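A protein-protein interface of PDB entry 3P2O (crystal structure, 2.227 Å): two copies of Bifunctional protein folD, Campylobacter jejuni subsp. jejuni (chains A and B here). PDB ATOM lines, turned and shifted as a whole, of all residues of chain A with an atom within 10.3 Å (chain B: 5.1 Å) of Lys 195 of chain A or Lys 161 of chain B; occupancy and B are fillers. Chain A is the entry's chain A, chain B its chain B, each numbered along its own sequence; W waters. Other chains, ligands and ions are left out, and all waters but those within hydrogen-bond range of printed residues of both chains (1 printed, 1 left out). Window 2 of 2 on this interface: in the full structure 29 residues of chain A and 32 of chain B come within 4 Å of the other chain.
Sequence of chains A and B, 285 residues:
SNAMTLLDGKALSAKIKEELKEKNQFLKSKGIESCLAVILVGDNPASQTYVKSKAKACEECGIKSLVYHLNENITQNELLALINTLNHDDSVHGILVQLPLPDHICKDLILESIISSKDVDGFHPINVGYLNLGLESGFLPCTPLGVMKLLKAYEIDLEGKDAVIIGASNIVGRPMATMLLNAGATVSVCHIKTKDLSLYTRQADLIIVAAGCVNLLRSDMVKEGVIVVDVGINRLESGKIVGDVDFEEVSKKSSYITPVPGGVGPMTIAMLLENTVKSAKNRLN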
ATOM      1  N   SER A 188     -26.302  25.922 -28.994  1.00  0.00           N
ATOM      2  CA  SER A 188     -25.344  24.892 -28.663  1.00  0.00           C
ATOM      3  C   SER A 188     -24.060  25.598 -28.286  1.00  0.00           C
ATOM      4  O   SER A 188     -23.615  26.498 -28.989  1.00  0.00           O
ATOM      5  CB  SER A 188     -25.096  23.954 -29.844  1.00  0.00           C
ATOM      6  OG  SER A 188     -26.317  23.398 -30.326  1.00  0.00           O
ATOM      7  N   VAL A 189     -23.454  25.172 -27.185  1.00  0.00           N
ATOM      8  CA  VAL A 189     -22.187  25.736 -26.792  1.00  0.00           C
ATOM      9  C   VAL A 189     -21.060  24.730 -26.921  1.00  0.00           C
ATOM     10  O   VAL A 189     -21.064  23.709 -26.240  1.00  0.00           O
ATOM     11  CB  VAL A 189     -22.217  26.250 -25.347  1.00  0.00           C
ATOM     12  CG1 VAL A 189     -20.859  26.892 -24.995  1.00  0.00           C
ATOM     13  CG2 VAL A 189     -23.405  27.209 -25.143  1.00  0.00           C
ATOM     14  N   CYS A 190     -20.081  25.061 -27.763  1.00  0.00           N
ATOM     15  CA  CYS A 190     -18.928  24.208 -27.995  1.00  0.00           C
ATOM     16  C   CYS A 190     -17.661  24.862 -27.493  1.00  0.00           C
ATOM     17  O   CYS A 190     -17.599  26.070 -27.307  1.00  0.00           O
ATOM     18  CB  CYS A 190     -18.782  23.885 -29.500  1.00  0.00           C
ATOM     19  SG  CYS A 190     -20.320  23.291 -30.299  1.00  0.00           S
ATOM     20  N   HIS A 191     -16.626  24.061 -27.327  1.00  0.00           N
ATOM     21  CA  HIS A 191     -15.374  24.574 -26.821  1.00  0.00           C
ATOM     22  C   HIS A 191     -14.308  23.542 -27.115  1.00  0.00           C
ATOM     23  O   HIS A 191     -14.569  22.553 -27.800  1.00  0.00           O
ATOM     24  CB  HIS A 191     -15.510  24.812 -25.317  1.00  0.00           C
ATOM     25  CG  HIS A 191     -16.230  23.713 -24.614  1.00  0.00           C
ATOM     26  ND1 HIS A 191     -15.598  22.560 -24.203  1.00  0.00           N
ATOM     27  CD2 HIS A 191     -17.536  23.568 -24.282  1.00  0.00           C
ATOM     28  CE1 HIS A 191     -16.475  21.759 -23.629  1.00  0.00           C
ATOM     29  NE2 HIS A 191     -17.661  22.341 -23.671  1.00  0.00           N
ATOM     30  N   ILE A 192     -13.124  23.748 -26.560  1.00  0.00           N
ATOM     31  CA  ILE A 192     -11.966  22.961 -26.937  1.00  0.00           C
ATOM     32  C   ILE A 192     -12.169  21.465 -26.670  1.00  0.00           C
ATOM     33  O   ILE A 192     -11.531  20.610 -27.310  1.00  0.00           O
ATOM     34  CB  ILE A 192     -10.690  23.479 -26.250  1.00  0.00           C
ATOM     35  CG1 ILE A 192      -9.455  22.797 -26.838  1.00  0.00           C
ATOM     36  CG2 ILE A 192     -10.788  23.315 -24.739  1.00  0.00           C
ATOM     37  CD1 ILE A 192      -8.794  23.589 -27.974  1.00  0.00           C
ATOM     38  N   LYS A 193     -13.063  21.137 -25.748  1.00  0.00           N
ATOM     39  CA  LYS A 193     -13.291  19.724 -25.444  1.00  0.00           C
ATOM     40  C   LYS A 193     -14.383  19.097 -26.328  1.00  0.00           C
ATOM     41  O   LYS A 193     -14.643  17.900 -26.230  1.00  0.00           O
ATOM     42  CB  LYS A 193     -13.587  19.498 -23.952  1.00  0.00           C
ATOM     43  CG  LYS A 193     -12.578  20.104 -22.966  1.00  0.00           C
ATOM     44  CD  LYS A 193     -11.187  19.521 -23.142  1.00  0.00           C
ATOM     45  CE  LYS A 193     -11.122  18.071 -22.671  1.00  0.00           C
ATOM     46  NZ  LYS A 193     -10.054  17.248 -23.335  1.00  0.00           N
ATOM     47  N   THR A 194     -15.013  19.882 -27.201  1.00  0.00           N
ATOM     48  CA  THR A 194     -16.036  19.291 -28.062  1.00  0.00           C
ATOM     49  C   THR A 194     -15.413  18.219 -28.979  1.00  0.00           C
ATOM     50  O   THR A 194     -14.318  18.413 -29.541  1.00  0.00           O
ATOM     51  CB  THR A 194     -16.777  20.337 -28.906  1.00  0.00           C
ATOM     52  OG1 THR A 194     -17.333  21.333 -28.050  1.00  0.00           O
ATOM     53  CG2 THR A 194     -17.919  19.680 -29.690  1.00  0.00           C
ATOM     54  N   LYS A 195     -16.102  17.085 -29.107  1.00  0.00           N
ATOM     55  CA  LYS A 195     -15.600  15.964 -29.889  1.00  0.00           C
ATOM     56  C   LYS A 195     -15.530  16.339 -31.364  1.00  0.00           C
ATOM     57  O   LYS A 195     -14.531  16.054 -32.035  1.00  0.00           O
ATOM     58  CB  LYS A 195     -16.457  14.704 -29.678  1.00  0.00           C
ATOM     59  CG  LYS A 195     -16.430  14.228 -28.228  1.00  0.00           C
ATOM     60  CD  LYS A 195     -16.950  12.813 -28.021  1.00  0.00           C
ATOM     61  CE  LYS A 195     -18.465  12.752 -27.874  1.00  0.00           C
ATOM     62  NZ  LYS A 195     -18.898  11.379 -27.404  1.00  0.00           N
ATOM     63  N   ASP A 196     -16.569  17.005 -31.859  1.00  0.00           N
ATOM     64  CA  ASP A 196     -16.662  17.257 -33.294  1.00  0.00           C
ATOM     65  C   ASP A 196     -17.542  18.451 -33.574  1.00  0.00           C
ATOM     66  O   ASP A 196     -18.764  18.377 -33.511  1.00  0.00           O
ATOM     67  CB  ASP A 196     -17.204  16.011 -34.018  1.00  0.00           C
ATOM     68  CG  ASP A 196     -17.260  16.174 -35.540  1.00  0.00           C
ATOM     69  OD1 ASP A 196     -17.014  17.292 -36.057  1.00  0.00           O
ATOM     70  OD2 ASP A 196     -17.578  15.161 -36.216  1.00  0.00           O
ATOM     71  N   LEU A 197     -16.891  19.549 -33.915  1.00  0.00           N
ATOM     72  CA  LEU A 197     -17.537  20.834 -34.153  1.00  0.00           C
ATOM     73  C   LEU A 197     -18.525  20.841 -35.336  1.00  0.00           C
ATOM     74  O   LEU A 197     -19.566  21.510 -35.285  1.00  0.00           O
ATOM     75  CB  LEU A 197     -16.431  21.867 -34.402  1.00  0.00           C
ATOM     76  CG  LEU A 197     -16.270  23.172 -33.648  1.00  0.00           C
ATOM     77  CD1 LEU A 197     -16.602  23.031 -32.165  1.00  0.00           C
ATOM     78  CD2 LEU A 197     -14.834  23.652 -33.850  1.00  0.00           C
ATOM     79  N   SER A 198     -18.195  20.126 -36.415  1.00  0.00           N
ATOM     80  CA  SER A 198     -19.053  20.131 -37.610  1.00  0.00           C
ATOM     81  C   SER A 198     -20.405  19.482 -37.340  1.00  0.00           C
ATOM     82  O   SER A 198     -21.407  19.823 -37.977  1.00  0.00           O
ATOM     83  CB  SER A 198     -18.348  19.465 -38.808  1.00  0.00           C
ATOM     84  OG  SER A 198     -17.834  18.199 -38.430  1.00  0.00           O
ATOM     85  N   LEU A 199     -20.431  18.561 -36.382  1.00  0.00           N
ATOM     86  CA  LEU A 199     -21.692  17.999 -35.925  1.00  0.00           C
ATOM     87  C   LEU A 199     -22.687  19.129 -35.695  1.00  0.00           C
ATOM     88  O   LEU A 199     -23.835  19.048 -36.135  1.00  0.00           O
ATOM     89  CB  LEU A 199     -21.515  17.176 -34.638  1.00  0.00           C
ATOM     90  CG  LEU A 199     -22.773  16.420 -34.179  1.00  0.00           C
ATOM     91  CD1 LEU A 199     -22.917  15.085 -34.941  1.00  0.00           C
ATOM     92  CD2 LEU A 199     -22.820  16.190 -32.650  1.00  0.00           C
ATOM     93  N   TYR A 200     -22.237  20.187 -35.016  1.00  0.00           N
ATOM     94  CA  TYR A 200     -23.109  21.317 -34.672  1.00  0.00           C
ATOM     95  C   TYR A 200     -23.173  22.384 -35.773  1.00  0.00           C
ATOM     96  O   TYR A 200     -24.231  22.997 -35.997  1.00  0.00           O
ATOM     97  CB  TYR A 200     -22.666  21.977 -33.338  1.00  0.00           C
ATOM     98  CG  TYR A 200     -22.770  21.037 -32.168  1.00  0.00           C
ATOM     99  CD1 TYR A 200     -23.995  20.827 -31.528  1.00  0.00           C
ATOM    100  CD2 TYR A 200     -21.673  20.300 -31.758  1.00  0.00           C
ATOM    101  CE1 TYR A 200     -24.106  19.918 -30.480  1.00  0.00           C
ATOM    102  CE2 TYR A 200     -21.768  19.395 -30.717  1.00  0.00           C
ATOM    103  CZ  TYR A 200     -22.981  19.216 -30.076  1.00  0.00           C
ATOM    104  OH  TYR A 200     -23.065  18.325 -29.047  1.00  0.00           O
ATOM    105  N   ARG A 202     -22.612  22.346 -39.191  1.00  0.00           N
ATOM    106  CA  ARG A 202     -23.223  22.041 -40.489  1.00  0.00           C
ATOM    107  C   ARG A 202     -24.718  22.366 -40.512  1.00  0.00           C
ATOM    108  O   ARG A 202     -25.286  22.671 -41.560  1.00  0.00           O
ATOM    109  CB  ARG A 202     -22.989  20.573 -40.860  1.00  0.00           C
ATOM    110  CG  ARG A 202     -21.711  20.335 -41.670  1.00  0.00           C
ATOM    111  CD  ARG A 202     -21.613  18.882 -42.160  1.00  0.00           C
ATOM    112  NE  ARG A 202     -21.622  17.948 -41.032  1.00  0.00           N
ATOM    113  CZ  ARG A 202     -20.584  17.197 -40.676  1.00  0.00           C
ATOM    114  NH1 ARG A 202     -19.455  17.263 -41.381  1.00  0.00           N
ATOM    115  NH2 ARG A 202     -20.676  16.381 -39.625  1.00  0.00           N
ATOM    116  N   LEU A 216     -10.583  28.284 -37.582  1.00  0.00           N
ATOM    117  CA  LEU A 216     -11.344  27.259 -36.873  1.00  0.00           C
ATOM    118  C   LEU A 216     -12.615  26.913 -37.657  1.00  0.00           C
ATOM    119  O   LEU A 216     -13.117  25.794 -37.598  1.00  0.00           O
ATOM    120  CB  LEU A 216     -11.705  27.742 -35.445  1.00  0.00           C
ATOM    121  CG  LEU A 216     -12.409  26.778 -34.484  1.00  0.00           C
ATOM    122  CD1 LEU A 216     -11.773  25.361 -34.501  1.00  0.00           C
ATOM    123  CD2 LEU A 216     -12.420  27.353 -33.052  1.00  0.00           C
ATOM    124  N   MET A 221     -17.735  23.330 -43.055  1.00  0.00           N
ATOM    125  CA  MET A 221     -18.370  23.095 -41.761  1.00  0.00           C
ATOM    126  C   MET A 221     -19.731  23.766 -41.719  1.00  0.00           C
ATOM    127  O   MET A 221     -20.526  23.551 -40.787  1.00  0.00           O
ATOM    128  CB  MET A 221     -17.477  23.606 -40.625  1.00  0.00           C
ATOM    129  CG  MET A 221     -16.207  22.794 -40.479  1.00  0.00           C
ATOM    130  SD  MET A 221     -14.791  23.677 -39.487  1.00  0.00           S
ATOM    131  CE  MET A 221     -15.411  23.273 -37.665  1.00  0.00           C
ATOM    132  N   ASP B 157     -18.575   9.759 -16.703  1.00  0.00           N
ATOM    133  CA  ASP B 157     -17.718  10.874 -17.102  1.00  0.00           C
ATOM    134  C   ASP B 157     -18.491  11.812 -18.032  1.00  0.00           C
ATOM    135  O   ASP B 157     -19.260  11.352 -18.877  1.00  0.00           O
ATOM    136  CB  ASP B 157     -16.418  10.398 -17.764  1.00  0.00           C
ATOM    137  CG  ASP B 157     -15.447  11.560 -18.053  1.00  0.00           C
ATOM    138  OD1 ASP B 157     -15.417  12.537 -17.263  1.00  0.00           O
ATOM    139  OD2 ASP B 157     -14.720  11.502 -19.074  1.00  0.00           O
ATOM    140  N   LEU B 158     -18.296  13.124 -17.863  1.00  0.00           N
ATOM    141  CA  LEU B 158     -19.083  14.114 -18.589  1.00  0.00           C
ATOM    142  C   LEU B 158     -18.235  14.960 -19.535  1.00  0.00           C
ATOM    143  O   LEU B 158     -18.750  15.550 -20.484  1.00  0.00           O
ATOM    144  CB  LEU B 158     -19.811  15.038 -17.608  1.00  0.00           C
ATOM    145  CG  LEU B 158     -20.698  14.364 -16.552  1.00  0.00           C
ATOM    146  CD1 LEU B 158     -21.267  15.403 -15.611  1.00  0.00           C
ATOM    147  CD2 LEU B 158     -21.812  13.587 -17.208  1.00  0.00           C
ATOM    148  N   GLU B 159     -16.943  15.047 -19.259  1.00  0.00           N
ATOM    149  CA  GLU B 159     -16.068  15.857 -20.075  1.00  0.00           C
ATOM    150  C   GLU B 159     -16.171  15.391 -21.537  1.00  0.00           C
ATOM    151  O   GLU B 159     -15.951  14.218 -21.845  1.00  0.00           O
ATOM    152  CB  GLU B 159     -14.643  15.723 -19.539  1.00  0.00           C
ATOM    153  CG  GLU B 159     -13.592  16.688 -20.082  1.00  0.00           C
ATOM    154  CD  GLU B 159     -12.200  16.273 -19.620  1.00  0.00           C
ATOM    155  OE1 GLU B 159     -11.217  16.483 -20.361  1.00  0.00           O
ATOM    156  OE2 GLU B 159     -12.094  15.701 -18.509  1.00  0.00           O
ATOM    157  N   GLY B 160     -16.546  16.309 -22.427  1.00  0.00           N
ATOM    158  CA  GLY B 160     -16.562  16.028 -23.849  1.00  0.00           C
ATOM    159  C   GLY B 160     -17.864  15.443 -24.354  1.00  0.00           C
ATOM    160  O   GLY B 160     -18.038  15.317 -25.569  1.00  0.00           O
ATOM    161  N   LYS B 161     -18.777  15.069 -23.452  1.00  0.00           N
ATOM    162  CA  LYS B 161     -20.010  14.424 -23.911  1.00  0.00           C
ATOM    163  C   LYS B 161     -20.843  15.396 -24.736  1.00  0.00           C
ATOM    164  O   LYS B 161     -20.670  16.606 -24.625  1.00  0.00           O
ATOM    165  CB  LYS B 161     -20.817  13.819 -22.762  1.00  0.00           C
ATOM    166  CG  LYS B 161     -20.174  12.570 -22.179  1.00  0.00           C
ATOM    167  CD  LYS B 161     -19.630  11.675 -23.299  1.00  0.00           C
ATOM    168  CE  LYS B 161     -18.908  10.446 -22.766  1.00  0.00           C
ATOM    169  NZ  LYS B 161     -18.221   9.696 -23.874  1.00  0.00           N
ATOM    170  N   ASP B 162     -21.698  14.866 -25.604  1.00  0.00           N
ATOM    171  CA  ASP B 162     -22.646  15.689 -26.331  1.00  0.00           C
ATOM    172  C   ASP B 162     -23.956  15.679 -25.564  1.00  0.00           C
ATOM    173  O   ASP B 162     -24.696  14.687 -25.562  1.00  0.00           O
ATOM    174  CB  ASP B 162     -22.851  15.199 -27.766  1.00  0.00           C
ATOM    175  CG  ASP B 162     -21.612  15.412 -28.650  1.00  0.00           C
ATOM    176  OD1 ASP B 162     -21.005  16.506 -28.621  1.00  0.00           O
ATOM    177  OD2 ASP B 162     -21.244  14.470 -29.386  1.00  0.00           O
ATOM    178  N   ALA B 163     -24.233  16.789 -24.886  1.00  0.00           N
ATOM    179  CA  ALA B 163     -25.383  16.840 -24.003  1.00  0.00           C
ATOM    180  C   ALA B 163     -26.482  17.732 -24.544  1.00  0.00           C
ATOM    181  O   ALA B 163     -26.224  18.753 -25.160  1.00  0.00           O
ATOM    182  CB  ALA B 163     -24.966  17.255 -22.610  1.00  0.00           C
ATOM    183  N   GLY B 184     -17.333  20.282 -18.430  1.00  0.00           N
ATOM    184  CA  GLY B 184     -16.624  20.025 -19.682  1.00  0.00           C
ATOM    185  C   GLY B 184     -17.461  19.454 -20.821  1.00  0.00           C
ATOM    186  O   GLY B 184     -16.934  19.081 -21.861  1.00  0.00           O
ATOM    187  N   ALA B 185     -18.773  19.371 -20.626  1.00  0.00           N
ATOM    188  CA  ALA B 185     -19.659  18.828 -21.651  1.00  0.00           C
ATOM    189  C   ALA B 185     -19.935  19.866 -22.724  1.00  0.00           C
ATOM    190  O   ALA B 185     -19.810  21.080 -22.490  1.00  0.00           O
ATOM    191  CB  ALA B 185     -20.970  18.391 -21.029  1.00  0.00           C
ATOM    192  N   THR B 186     -20.338  19.397 -23.898  1.00  0.00           N
ATOM    193  CA  THR B 186     -20.849  20.289 -24.929  1.00  0.00           C
ATOM    194  C   THR B 186     -22.332  20.314 -24.678  1.00  0.00           C
ATOM    195  O   THR B 186     -22.921  19.249 -24.494  1.00  0.00           O
ATOM    196  CB  THR B 186     -20.560  19.733 -26.366  1.00  0.00           C
ATOM    197  OG1 THR B 186     -19.147  19.693 -26.561  1.00  0.00           O
ATOM    198  CG2 THR B 186     -21.210  20.625 -27.444  1.00  0.00           C
ATOM    199  N   ASP B 205     -25.214  12.083 -26.561  1.00  0.00           N
ATOM    200  CA  ASP B 205     -24.764  11.044 -25.640  1.00  0.00           C
ATOM    201  C   ASP B 205     -25.649  11.077 -24.392  1.00  0.00           C
ATOM    202  O   ASP B 205     -26.017  10.035 -23.866  1.00  0.00           O
ATOM    203  CB  ASP B 205     -23.309  11.283 -25.216  1.00  0.00           C
ATOM    204  CG  ASP B 205     -22.341  11.336 -26.403  1.00  0.00           C
ATOM    205  OD1 ASP B 205     -22.523  10.563 -27.377  1.00  0.00           O
ATOM    206  OD2 ASP B 205     -21.387  12.151 -26.355  1.00  0.00           O
HETATM  207  O   HOH W   1     -25.496  18.439 -27.861  1.00  0.00           O
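O of Val 189 of chain A touches CG2 of Thr 186 of chain B, at 3.3 Å.
Gly 184 of chain B touches His 191 of chain A (O to CE1, 3.2 Å).
N of Thr 186 of chain B touches NE2 of His 191 of chain A (3.99 Å).
Gly 160 of chain B touches Lys 193 of chain A (CA to O, 3.6 Å).
O of Gly 184 of chain B touches CB of Lys 193 of chain A (3.97 Å).
CG of Lys 195 of chain A touches O of Gly 160 of chain B, at 3.3 Å.
Lys 195 of chain A touches Lys 161 of chain B (NZ to NZ, 3.97 Å).
CE of Lys 195 of chain A touches OD2 of Asp 162 of chain B, 3.6 Å away.
Thr 186 of chain B touches Tyr 200 of chain A (CG2 to OH, 3.4 Å).
Hydrophobic or aromatic side chains of chain A within 4 Å of the printed part of chain B: His 191 and Tyr 200.
Along chain A the printed residues that touch a printed residue of chain B span positions 189 to 200.
Of the 11 printed residues of chain B, 8 touch a printed residue of chain A.
Printed residues of chain B that touch a printed residue of chain A: Glu 159, Gly 160, Lys 161, Asp 162, Gly 184, Ala 185, Thr 186 and Asp 205.
Among the printed residues, Asp or Glu carboxylates within 4 Å of a Lys or Arg side-chain nitrogen of the other chain: Lys 193 of chain A with Glu 159 of chain B and Lys 195 of chain A with Asp 205 of chain B.
OD2 of Asp 205 of chain B lies within hydrogen-bond range of N of Asp 162 of chain B, 2.8 Å away.
The backbone carbonyl oxygen of Thr 186 of chain B lies within hydrogen-bond range of the backbone NH of Ala 163 of chain B (2.8 Å).
The backbone carbonyl oxygen (O) of Lys 161 of chain B lies within hydrogen-bond range of the backbone NH (N) of Thr 186 of chain B (2.9 Å).
OG1 of Thr 194 of chain A lies within hydrogen-bond range of N of His 191 of chain A.
The backbone NH of Gly 160 of chain B is in hydrogen-bond range of the backbone carbonyl oxygen of Gly 184 of chain B.
N of Lys 193 of chain A lies close to ND1 of His 191 of chain A (3.3 Å).
Lys 195 of chain A touches four residues of chain B.
Printed residues of chain A within 4 Å of Gly 160 of chain B: Lys 193 (3.6 Å) and Lys 195 (3.3 Å).
No residue of chain A comes within 4 Å of Ala 163 of chain B.
Ala 185 of chain B touches just one residue of chain A: His 191 (2.8 Å).
Printed residues of chain B within 4 Å of Tyr 200 of chain A: Asp 162 and Thr 186.
Printed residues of chain A within 4 Å of Thr 186 of chain B: Val 189, His 191, Thr 194 and Tyr 200.
Printed residues of chain B within 4 Å of His 191 of chain A: Gly 184 (3.2 Å), Ala 185 (2.8 Å) and Thr 186 (3.99 Å).
Printed residues of chain A within 4 Å of Glu 159 of chain B: Lys 193 (2.8 Å).
Of the printed residues of chain B, Thr 194 of chain A touches Thr 186 (2.9 Å).
The nearest residue of chain B that does not touch Lys 195 of chain A is Thr 186 of chain B (4.7 Å).
O of Ala 185 of chain B sits at hydrogen-bond distance from NE2 of His 191 of chain A (2.8 Å).
NZ of Lys 193 of chain A lies within salt-bridge range of OE1 of Glu 159 of chain B, at 3.3 Å.
The side-chain hydroxyl (OH) of Tyr 200 of chain A lies within hydrogen-bond range of the side-chain carboxylate (OD1) of Asp 162 of chain B (2.8 Å).
NZ of Lys 195 of chain A lies within salt-bridge range of OD2 of Asp 205 of chain B, 2.8 Å away.
The side-chain hydroxyl (OG1) of Thr 186 of chain B sits at hydrogen-bond distance from the side-chain hydroxyl (OG1) of Thr 194 of chain A (2.9 Å).
No position is printed for both chains.
Of the 14 pairs that touch across the chains among the printed residues, none has its exchanged pair printed and touching as well.
Water W1 lies within hydrogen-bond range of OH of Tyr 200 of chain A (2.7 Å) and O of Ala 163 of chain B (2.8 Å).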
